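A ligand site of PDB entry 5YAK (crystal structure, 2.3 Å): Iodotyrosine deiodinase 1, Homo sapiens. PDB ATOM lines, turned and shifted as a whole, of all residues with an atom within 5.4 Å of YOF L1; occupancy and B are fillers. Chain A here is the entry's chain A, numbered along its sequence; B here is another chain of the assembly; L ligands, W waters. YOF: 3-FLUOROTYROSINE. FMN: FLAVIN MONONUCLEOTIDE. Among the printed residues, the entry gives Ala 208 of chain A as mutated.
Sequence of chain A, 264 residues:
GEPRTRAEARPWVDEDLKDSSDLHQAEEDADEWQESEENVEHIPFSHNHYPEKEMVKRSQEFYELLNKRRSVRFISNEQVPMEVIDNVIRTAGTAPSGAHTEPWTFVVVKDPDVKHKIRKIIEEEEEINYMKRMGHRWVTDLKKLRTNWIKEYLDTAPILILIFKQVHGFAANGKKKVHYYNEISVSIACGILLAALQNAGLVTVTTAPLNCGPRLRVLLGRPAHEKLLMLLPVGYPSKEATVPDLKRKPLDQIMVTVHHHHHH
Water W3 bridges O of YOF L1 (2.8 Å) and OE2 of Glu 126 (2.9 Å).
Water W1 lies within hydrogen-bond range of the side-chain hydroxyl (OH) of Tyr 181 of chain B (2.8 Å), a nitrogen (N) of YOF L1 (2.9 Å) and the backbone carbonyl oxygen (O) of Ala 208 (3.0 Å).
Water W2 lies within hydrogen-bond range of the side-chain carboxylate of Glu 126 (2.7 Å), a nitrogen (N) of YOF L1 (3.1 Å) and the side-chain sulfur of Met 134 (3.5 Å).
A nitrogen (N) of YOF L1 is in hydrogen-bond range of an oxygen (O4) of FMN L2.
O of Asn 148 sits close to OXT of YOF L1, 3.5 Å away.
Trp 138 touches YOF L1.
Leu 142 touches YOF L1.
Leu 145 touches YOF L1 (CD1 to F, 3.8 Å).
Thr 147 touches YOF L1.
Ala 208 touches YOF L1 (O to N, 3.7 Å).
Gly 98 of chain B touches YOF L1 (CA to OH, 3.3 Å).
Tyr 180 of chain B touches YOF L1 (CB to OH, 3.999 Å).
Tyr 181 of chain B touches YOF L1 (CD1 to OH, 3.6 Å).
Hydrophobic or aromatic side chains within 4 Å of YOF L1: Tyr 130, Trp 138, Leu 142, Leu 145, Tyr 180 of chain B and Tyr 181 of chain B.
Of the 21 residues printed, 13 come within 4 Å of YOF L1.
The nearest printed residue that does not touch YOF L1 is Met 134 (4.2 Å).
The guanidinium group (NE) of Arg 73 lies within hydrogen-bond range of an oxygen (O2) of FMN L2 (2.8 Å).
OH of Tyr 130 sits at hydrogen-bond distance from OXT of YOF L1 (2.6 Å).
An oxygen (OH) of YOF L1 sits at hydrogen-bond distance from the backbone NH of Ala 99 of chain B, at 3.2 Å.
The backbone NH (N) of Ser 97 of chain B is in hydrogen-bond range of an oxygen (O3') of FMN L2, at 3.1 Å.
The side-chain carboxylate (OE2) of Glu 126 is in salt-bridge range of a nitrogen (N) of YOF L1 (3.0 Å).
N of Ala 208 lies within hydrogen-bond range of O4 of FMN L2 (3.0 Å).
OXT of YOF L1 lies within salt-bridge range of NZ of Lys 151 (2.6 Å).
O of Asn 148 is in hydrogen-bond range of NZ of Lys 151 (2.7 Å).
OG1 of Thr 147 is in hydrogen-bond range of OH of Tyr 130 (2.9 Å).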
ATOM      1  N   ARG A  73     -24.387 -12.568 -24.134  1.00  0.00           N
ATOM      2  CA  ARG A  73     -24.132 -11.832 -25.350  1.00  0.00           C
ATOM      3  C   ARG A  73     -23.120 -12.527 -26.277  1.00  0.00           C
ATOM      4  O   ARG A  73     -22.655 -11.920 -27.238  1.00  0.00           O
ATOM      5  CB  ARG A  73     -23.650 -10.426 -25.004  1.00  0.00           C
ATOM      6  CG  ARG A  73     -24.706  -9.639 -24.283  1.00  0.00           C
ATOM      7  CD  ARG A  73     -24.219  -8.301 -23.825  1.00  0.00           C
ATOM      8  NE  ARG A  73     -25.348  -7.602 -23.274  1.00  0.00           N
ATOM      9  CZ  ARG A  73     -25.610  -7.497 -21.980  1.00  0.00           C
ATOM     10  NH1 ARG A  73     -24.790  -8.007 -21.034  1.00  0.00           N
ATOM     11  NH2 ARG A  73     -26.718  -6.871 -21.614  1.00  0.00           N
ATOM     12  N   GLU A 126     -26.986   1.389 -34.049  1.00  0.00           N
ATOM     13  CA  GLU A 126     -26.441   1.458 -32.680  1.00  0.00           C
ATOM     14  C   GLU A 126     -25.176   2.308 -32.603  1.00  0.00           C
ATOM     15  O   GLU A 126     -24.955   3.025 -31.609  1.00  0.00           O
ATOM     16  CB  GLU A 126     -26.184   0.057 -32.102  1.00  0.00           C
ATOM     17  CG  GLU A 126     -27.468  -0.738 -31.864  1.00  0.00           C
ATOM     18  CD  GLU A 126     -28.235  -0.350 -30.606  1.00  0.00           C
ATOM     19  OE1 GLU A 126     -28.064   0.766 -30.091  1.00  0.00           O
ATOM     20  OE2 GLU A 126     -29.007  -1.187 -30.113  1.00  0.00           O
ATOM     21  N   TYR A 130     -24.924   5.212 -29.937  1.00  0.00           N
ATOM     22  CA  TYR A 130     -23.849   5.372 -28.934  1.00  0.00           C
ATOM     23  C   TYR A 130     -23.123   6.706 -29.119  1.00  0.00           C
ATOM     24  O   TYR A 130     -22.665   7.295 -28.122  1.00  0.00           O
ATOM     25  CB  TYR A 130     -22.830   4.220 -28.977  1.00  0.00           C
ATOM     26  CG  TYR A 130     -23.199   3.048 -28.123  1.00  0.00           C
ATOM     27  CD1 TYR A 130     -22.743   2.927 -26.823  1.00  0.00           C
ATOM     28  CD2 TYR A 130     -24.066   2.075 -28.604  1.00  0.00           C
ATOM     29  CE1 TYR A 130     -23.126   1.877 -26.042  1.00  0.00           C
ATOM     30  CE2 TYR A 130     -24.455   1.013 -27.827  1.00  0.00           C
ATOM     31  CZ  TYR A 130     -23.977   0.913 -26.560  1.00  0.00           C
ATOM     32  OH  TYR A 130     -24.378  -0.169 -25.809  1.00  0.00           O
ATOM     33  N   MET A 134     -28.323   8.406 -27.823  1.00  0.00           N
ATOM     34  CA  MET A 134     -28.634   7.954 -26.431  1.00  0.00           C
ATOM     35  C   MET A 134     -28.318   9.001 -25.394  1.00  0.00           C
ATOM     36  O   MET A 134     -29.017   9.106 -24.372  1.00  0.00           O
ATOM     37  CB  MET A 134     -27.874   6.637 -26.070  1.00  0.00           C
ATOM     38  CG  MET A 134     -28.332   5.379 -26.828  1.00  0.00           C
ATOM     39  SD  MET A 134     -27.081   4.055 -27.010  1.00  0.00           S
ATOM     40  CE  MET A 134     -27.192   3.488 -25.331  1.00  0.00           C
ATOM     41  N   TRP A 138     -26.738   7.797 -20.471  1.00  0.00           N
ATOM     42  CA  TRP A 138     -27.157   6.465 -20.856  1.00  0.00           C
ATOM     43  C   TRP A 138     -25.897   5.656 -21.201  1.00  0.00           C
ATOM     44  O   TRP A 138     -25.729   4.520 -20.743  1.00  0.00           O
ATOM     45  CB  TRP A 138     -28.134   6.532 -22.040  1.00  0.00           C
ATOM     46  CG  TRP A 138     -28.807   5.234 -22.385  1.00  0.00           C
ATOM     47  CD1 TRP A 138     -28.497   4.007 -21.912  1.00  0.00           C
ATOM     48  CD2 TRP A 138     -29.892   5.050 -23.312  1.00  0.00           C
ATOM     49  NE1 TRP A 138     -29.334   3.050 -22.457  1.00  0.00           N
ATOM     50  CE2 TRP A 138     -30.205   3.671 -23.319  1.00  0.00           C
ATOM     51  CE3 TRP A 138     -30.640   5.913 -24.123  1.00  0.00           C
ATOM     52  CZ2 TRP A 138     -31.224   3.130 -24.115  1.00  0.00           C
ATOM     53  CZ3 TRP A 138     -31.670   5.369 -24.910  1.00  0.00           C
ATOM     54  CH2 TRP A 138     -31.957   3.992 -24.893  1.00  0.00           C
ATOM     55  N   LEU A 142     -24.190   2.266 -19.210  1.00  0.00           N
ATOM     56  CA  LEU A 142     -23.886   0.971 -19.818  1.00  0.00           C
ATOM     57  C   LEU A 142     -22.452   0.485 -19.709  1.00  0.00           C
ATOM     58  O   LEU A 142     -22.162  -0.644 -20.114  1.00  0.00           O
ATOM     59  CB  LEU A 142     -24.249   0.975 -21.300  1.00  0.00           C
ATOM     60  CG  LEU A 142     -25.715   1.272 -21.674  1.00  0.00           C
ATOM     61  CD1 LEU A 142     -25.898   1.242 -23.186  1.00  0.00           C
ATOM     62  CD2 LEU A 142     -26.643   0.246 -21.012  1.00  0.00           C
ATOM     63  N   LEU A 145     -21.662  -2.990 -18.385  1.00  0.00           N
ATOM     64  CA  LEU A 145     -22.100  -4.136 -19.161  1.00  0.00           C
ATOM     65  C   LEU A 145     -21.145  -4.336 -20.315  1.00  0.00           C
ATOM     66  O   LEU A 145     -21.155  -5.398 -20.919  1.00  0.00           O
ATOM     67  CB  LEU A 145     -23.513  -3.927 -19.707  1.00  0.00           C
ATOM     68  CG  LEU A 145     -24.626  -3.643 -18.694  1.00  0.00           C
ATOM     69  CD1 LEU A 145     -25.981  -3.413 -19.351  1.00  0.00           C
ATOM     70  CD2 LEU A 145     -24.735  -4.789 -17.704  1.00  0.00           C
ATOM     71  N   THR A 147     -21.230  -3.256 -23.319  1.00  0.00           N
ATOM     72  CA  THR A 147     -21.867  -3.241 -24.635  1.00  0.00           C
ATOM     73  C   THR A 147     -21.366  -2.073 -25.520  1.00  0.00           C
ATOM     74  O   THR A 147     -21.023  -1.004 -25.030  1.00  0.00           O
ATOM     75  CB  THR A 147     -23.379  -3.064 -24.462  1.00  0.00           C
ATOM     76  OG1 THR A 147     -23.611  -1.945 -23.587  1.00  0.00           O
ATOM     77  CG2 THR A 147     -23.992  -4.307 -23.833  1.00  0.00           C
ATOM     78  N   ASN A 148     -21.333  -2.306 -26.831  1.00  0.00           N
ATOM     79  CA  ASN A 148     -21.066  -1.239 -27.790  1.00  0.00           C
ATOM     80  C   ASN A 148     -21.938  -1.475 -29.002  1.00  0.00           C
ATOM     81  O   ASN A 148     -22.967  -2.159 -28.870  1.00  0.00           O
ATOM     82  CB  ASN A 148     -19.588  -1.241 -28.153  1.00  0.00           C
ATOM     83  CG  ASN A 148     -19.065  -2.627 -28.384  1.00  0.00           C
ATOM     84  OD1 ASN A 148     -19.560  -3.373 -29.220  1.00  0.00           O
ATOM     85  ND2 ASN A 148     -18.043  -2.985 -27.636  1.00  0.00           N
ATOM     86  N   LYS A 151     -22.312  -6.267 -32.734  1.00  0.00           N
ATOM     87  CA  LYS A 151     -23.299  -7.254 -32.301  1.00  0.00           C
ATOM     88  C   LYS A 151     -23.073  -8.525 -33.070  1.00  0.00           C
ATOM     89  O   LYS A 151     -23.898  -8.954 -33.868  1.00  0.00           O
ATOM     90  CB  LYS A 151     -24.726  -6.735 -32.485  1.00  0.00           C
ATOM     91  CG  LYS A 151     -25.015  -5.398 -31.785  1.00  0.00           C
ATOM     92  CD  LYS A 151     -24.791  -5.450 -30.282  1.00  0.00           C
ATOM     93  CE  LYS A 151     -25.307  -4.196 -29.611  1.00  0.00           C
ATOM     94  NZ  LYS A 151     -24.822  -4.022 -28.211  1.00  0.00           N
ATOM     95  N   TYR A 153     -23.257 -11.531 -32.169  1.00  0.00           N
ATOM     96  CA  TYR A 153     -24.242 -12.582 -31.942  1.00  0.00           C
ATOM     97  C   TYR A 153     -25.310 -12.656 -33.031  1.00  0.00           C
ATOM     98  O   TYR A 153     -25.932 -13.712 -33.223  1.00  0.00           O
ATOM     99  CB  TYR A 153     -24.852 -12.455 -30.543  1.00  0.00           C
ATOM    100  CG  TYR A 153     -25.487 -11.121 -30.214  1.00  0.00           C
ATOM    101  CD1 TYR A 153     -24.897 -10.271 -29.284  1.00  0.00           C
ATOM    102  CD2 TYR A 153     -26.696 -10.744 -30.771  1.00  0.00           C
ATOM    103  CE1 TYR A 153     -25.484  -9.061 -28.950  1.00  0.00           C
ATOM    104  CE2 TYR A 153     -27.281  -9.532 -30.447  1.00  0.00           C
ATOM    105  CZ  TYR A 153     -26.684  -8.698 -29.539  1.00  0.00           C
ATOM    106  OH  TYR A 153     -27.301  -7.496 -29.201  1.00  0.00           O
ATOM    107  N   THR A 207     -32.832  -7.862 -26.251  1.00  0.00           N
ATOM    108  CA  THR A 207     -32.365  -6.566 -26.780  1.00  0.00           C
ATOM    109  C   THR A 207     -33.446  -5.675 -27.359  1.00  0.00           C
ATOM    110  O   THR A 207     -34.431  -6.146 -27.921  1.00  0.00           O
ATOM    111  CB  THR A 207     -31.250  -6.741 -27.824  1.00  0.00           C
ATOM    112  OG1 THR A 207     -31.824  -7.235 -29.037  1.00  0.00           O
ATOM    113  CG2 THR A 207     -30.199  -7.701 -27.334  1.00  0.00           C
ATOM    114  N   ALA A 208     -33.208  -4.370 -27.252  1.00  0.00           N
ATOM    115  CA  ALA A 208     -34.086  -3.350 -27.788  1.00  0.00           C
ATOM    116  C   ALA A 208     -33.264  -2.476 -28.749  1.00  0.00           C
ATOM    117  O   ALA A 208     -32.704  -1.453 -28.357  1.00  0.00           O
ATOM    118  CB  ALA A 208     -34.668  -2.499 -26.675  1.00  0.00           C
ATOM    119  N   PRO A 209     -33.187  -2.890 -30.024  1.00  0.00           N
ATOM    120  CA  PRO A 209     -32.407  -2.138 -31.003  1.00  0.00           C
ATOM    121  C   PRO A 209     -33.091  -0.809 -31.392  1.00  0.00           C
ATOM    122  O   PRO A 209     -33.870  -0.745 -32.351  1.00  0.00           O
ATOM    123  CB  PRO A 209     -32.308  -3.114 -32.170  1.00  0.00           C
ATOM    124  CG  PRO A 209     -33.508  -4.008 -32.040  1.00  0.00           C
ATOM    125  CD  PRO A 209     -33.856  -4.073 -30.584  1.00  0.00           C
ATOM    126  N   LEU A 210     -32.774   0.236 -30.632  1.00  0.00           N
ATOM    127  CA  LEU A 210     -33.368   1.552 -30.763  1.00  0.00           C
ATOM    128  C   LEU A 210     -33.223   2.083 -32.197  1.00  0.00           C
ATOM    129  O   LEU A 210     -32.154   1.941 -32.821  1.00  0.00           O
ATOM    130  CB  LEU A 210     -32.657   2.480 -29.801  1.00  0.00           C
ATOM    131  CG  LEU A 210     -33.118   3.943 -29.710  1.00  0.00           C
ATOM    132  CD1 LEU A 210     -34.562   4.022 -29.237  1.00  0.00           C
ATOM    133  CD2 LEU A 210     -32.190   4.735 -28.791  1.00  0.00           C
ATOM    134  N   SER B  97     -33.587  -6.604 -16.997  1.00  0.00           N
ATOM    135  CA  SER B  97     -34.072  -5.218 -16.914  1.00  0.00           C
ATOM    136  C   SER B  97     -33.104  -4.279 -17.626  1.00  0.00           C
ATOM    137  O   SER B  97     -31.899  -4.497 -17.616  1.00  0.00           O
ATOM    138  CB  SER B  97     -34.308  -4.753 -15.469  1.00  0.00           C
ATOM    139  OG  SER B  97     -33.096  -4.616 -14.717  1.00  0.00           O
ATOM    140  N   GLY B  98     -33.656  -3.249 -18.243  1.00  0.00           N
ATOM    141  CA  GLY B  98     -32.859  -2.222 -18.925  1.00  0.00           C
ATOM    142  C   GLY B  98     -31.723  -1.690 -18.082  1.00  0.00           C
ATOM    143  O   GLY B  98     -31.945  -1.135 -17.030  1.00  0.00           O
ATOM    144  N   ALA B  99     -30.501  -1.885 -18.569  1.00  0.00           N
ATOM    145  CA  ALA B  99     -29.283  -1.447 -17.874  1.00  0.00           C
ATOM    146  C   ALA B  99     -29.191  -1.971 -16.434  1.00  0.00           C
ATOM    147  O   ALA B  99     -28.620  -1.304 -15.571  1.00  0.00           O
ATOM    148  CB  ALA B  99     -29.152   0.066 -17.891  1.00  0.00           C
ATOM    149  N   HIS B 100     -29.758  -3.152 -16.167  1.00  0.00           N
ATOM    150  CA  HIS B 100     -29.718  -3.738 -14.818  1.00  0.00           C
ATOM    151  C   HIS B 100     -30.195  -2.748 -13.767  1.00  0.00           C
ATOM    152  O   HIS B 100     -29.477  -2.441 -12.813  1.00  0.00           O
ATOM    153  CB  HIS B 100     -28.295  -4.225 -14.434  1.00  0.00           C
ATOM    154  CG  HIS B 100     -28.279  -5.045 -13.171  1.00  0.00           C
ATOM    155  ND1 HIS B 100     -29.188  -6.038 -12.922  1.00  0.00           N
ATOM    156  CD2 HIS B 100     -27.482  -4.976 -12.083  1.00  0.00           C
ATOM    157  CE1 HIS B 100     -28.966  -6.557 -11.729  1.00  0.00           C
ATOM    158  NE2 HIS B 100     -27.938  -5.924 -11.202  1.00  0.00           N
ATOM    159  N   TYR B 180     -34.169   2.737 -17.759  1.00  0.00           N
ATOM    160  CA  TYR B 180     -34.360   2.472 -19.171  1.00  0.00           C
ATOM    161  C   TYR B 180     -35.316   1.320 -19.359  1.00  0.00           C
ATOM    162  O   TYR B 180     -35.141   0.259 -18.752  1.00  0.00           O
ATOM    163  CB  TYR B 180     -32.995   2.123 -19.788  1.00  0.00           C
ATOM    164  CG  TYR B 180     -31.946   3.190 -19.499  1.00  0.00           C
ATOM    165  CD1 TYR B 180     -31.869   4.339 -20.267  1.00  0.00           C
ATOM    166  CD2 TYR B 180     -31.085   3.066 -18.405  1.00  0.00           C
ATOM    167  CE1 TYR B 180     -30.959   5.330 -19.982  1.00  0.00           C
ATOM    168  CE2 TYR B 180     -30.182   4.060 -18.079  1.00  0.00           C
ATOM    169  CZ  TYR B 180     -30.108   5.190 -18.871  1.00  0.00           C
ATOM    170  OH  TYR B 180     -29.220   6.201 -18.545  1.00  0.00           O
ATOM    171  N   TYR B 181     -36.288   1.534 -20.248  1.00  0.00           N
ATOM    172  CA  TYR B 181     -37.268   0.523 -20.588  1.00  0.00           C
ATOM    173  C   TYR B 181     -37.953  -0.006 -19.328  1.00  0.00           C
ATOM    174  O   TYR B 181     -38.091  -1.213 -19.206  1.00  0.00           O
ATOM    175  CB  TYR B 181     -36.620  -0.656 -21.329  1.00  0.00           C
ATOM    176  CG  TYR B 181     -35.989  -0.232 -22.615  1.00  0.00           C
ATOM    177  CD1 TYR B 181     -34.604  -0.208 -22.741  1.00  0.00           C
ATOM    178  CD2 TYR B 181     -36.760   0.215 -23.689  1.00  0.00           C
ATOM    179  CE1 TYR B 181     -34.001   0.221 -23.887  1.00  0.00           C
ATOM    180  CE2 TYR B 181     -36.152   0.638 -24.857  1.00  0.00           C
ATOM    181  CZ  TYR B 181     -34.773   0.655 -24.943  1.00  0.00           C
ATOM    182  OH  TYR B 181     -34.108   1.089 -26.089  1.00  0.00           O
HETATM  183  N   YOF L   1     -29.236  -1.177 -27.136  1.00  0.00           N
HETATM  184  CA  YOF L   1     -27.812  -0.914 -26.822  1.00  0.00           C
HETATM  185  C   YOF L   1     -27.039  -2.131 -27.139  1.00  0.00           C
HETATM  186  O   YOF L   1     -27.655  -3.165 -27.551  1.00  0.00           O
HETATM  187  OXT YOF L   1     -25.815  -2.071 -26.850  1.00  0.00           O
HETATM  188  CB  YOF L   1     -27.335  -0.737 -25.382  1.00  0.00           C
HETATM  189  CG  YOF L   1     -28.213  -1.152 -24.234  1.00  0.00           C
HETATM  190  CD1 YOF L   1     -28.122  -2.120 -23.192  1.00  0.00           C
HETATM  191  CD2 YOF L   1     -29.218  -0.265 -24.278  1.00  0.00           C
HETATM  192  CE1 YOF L   1     -29.190  -2.142 -22.217  1.00  0.00           C
HETATM  193  CE2 YOF L   1     -30.198  -0.310 -23.356  1.00  0.00           C
HETATM  194  CZ  YOF L   1     -30.211  -1.221 -22.381  1.00  0.00           C
HETATM  195  OH  YOF L   1     -31.268  -1.008 -21.578  1.00  0.00           O
HETATM  196  F   YOF L   1     -29.330  -2.955 -21.131  1.00  0.00           F
HETATM  197  N1  FMN L   2     -29.026  -5.914 -23.374  1.00  0.00           N
HETATM  198  C2  FMN L   2     -28.351  -5.526 -24.465  1.00  0.00           C
HETATM  199  O2  FMN L   2     -27.191  -5.946 -24.581  1.00  0.00           O
HETATM  200  N3  FMN L   2     -28.847  -4.639 -25.367  1.00  0.00           N
HETATM  201  C4  FMN L   2     -30.106  -4.139 -25.262  1.00  0.00           C
HETATM  202  O4  FMN L   2     -30.636  -3.355 -26.085  1.00  0.00           O
HETATM  203  C4A FMN L   2     -30.895  -4.545 -24.099  1.00  0.00           C
HETATM  204  N5  FMN L   2     -32.150  -4.090 -23.960  1.00  0.00           N
HETATM  205  C5A FMN L   2     -32.906  -4.530 -22.931  1.00  0.00           C
HETATM  206  C6  FMN L   2     -34.198  -4.058 -22.837  1.00  0.00           C
HETATM  207  C7  FMN L   2     -35.004  -4.499 -21.816  1.00  0.00           C
HETATM  208  C7M FMN L   2     -36.425  -4.060 -21.716  1.00  0.00           C
HETATM  209  C8  FMN L   2     -34.494  -5.495 -20.859  1.00  0.00           C
HETATM  210  C8M FMN L   2     -35.407  -5.972 -19.779  1.00  0.00           C
HETATM  211  C9  FMN L   2     -33.189  -5.918 -20.912  1.00  0.00           C
HETATM  212  C9A FMN L   2     -32.347  -5.499 -21.932  1.00  0.00           C
HETATM  213  N10 FMN L   2     -31.005  -5.958 -22.027  1.00  0.00           N
HETATM  214  C10 FMN L   2     -30.269  -5.501 -23.138  1.00  0.00           C
HETATM  215  C1' FMN L   2     -30.426  -6.924 -21.086  1.00  0.00           C
HETATM  216  C2' FMN L   2     -30.089  -6.226 -19.749  1.00  0.00           C
HETATM  217  O2' FMN L   2     -28.902  -5.427 -19.970  1.00  0.00           O
HETATM  218  C3' FMN L   2     -29.887  -7.292 -18.626  1.00  0.00           C
HETATM  219  O3' FMN L   2     -31.134  -7.926 -18.281  1.00  0.00           O
HETATM  220  C4' FMN L   2     -29.274  -6.757 -17.338  1.00  0.00           C
HETATM  221  O4' FMN L   2     -27.944  -6.249 -17.528  1.00  0.00           O
HETATM  222  C5' FMN L   2     -29.247  -7.768 -16.180  1.00  0.00           C
HETATM  223  O5' FMN L   2     -28.538  -8.943 -16.540  1.00  0.00           O
HETATM  224  P   FMN L   2     -29.268 -10.377 -16.539  1.00  0.00           P
HETATM  225  O1P FMN L   2     -29.914 -10.431 -15.177  1.00  0.00           O
HETATM  226  O2P FMN L   2     -30.307 -10.366 -17.660  1.00  0.00           O
HETATM  227  O3P FMN L   2     -28.113 -11.316 -16.892  1.00  0.00           O
HETATM  228  O   HOH W   1     -31.418   0.615 -26.620  1.00  0.00           O
HETATM  229  O   HOH W   2     -29.507   1.776 -28.105  1.00  0.00           O
HETATM  230  O   HOH W   3     -29.056  -4.051 -29.751  1.00  0.00           O
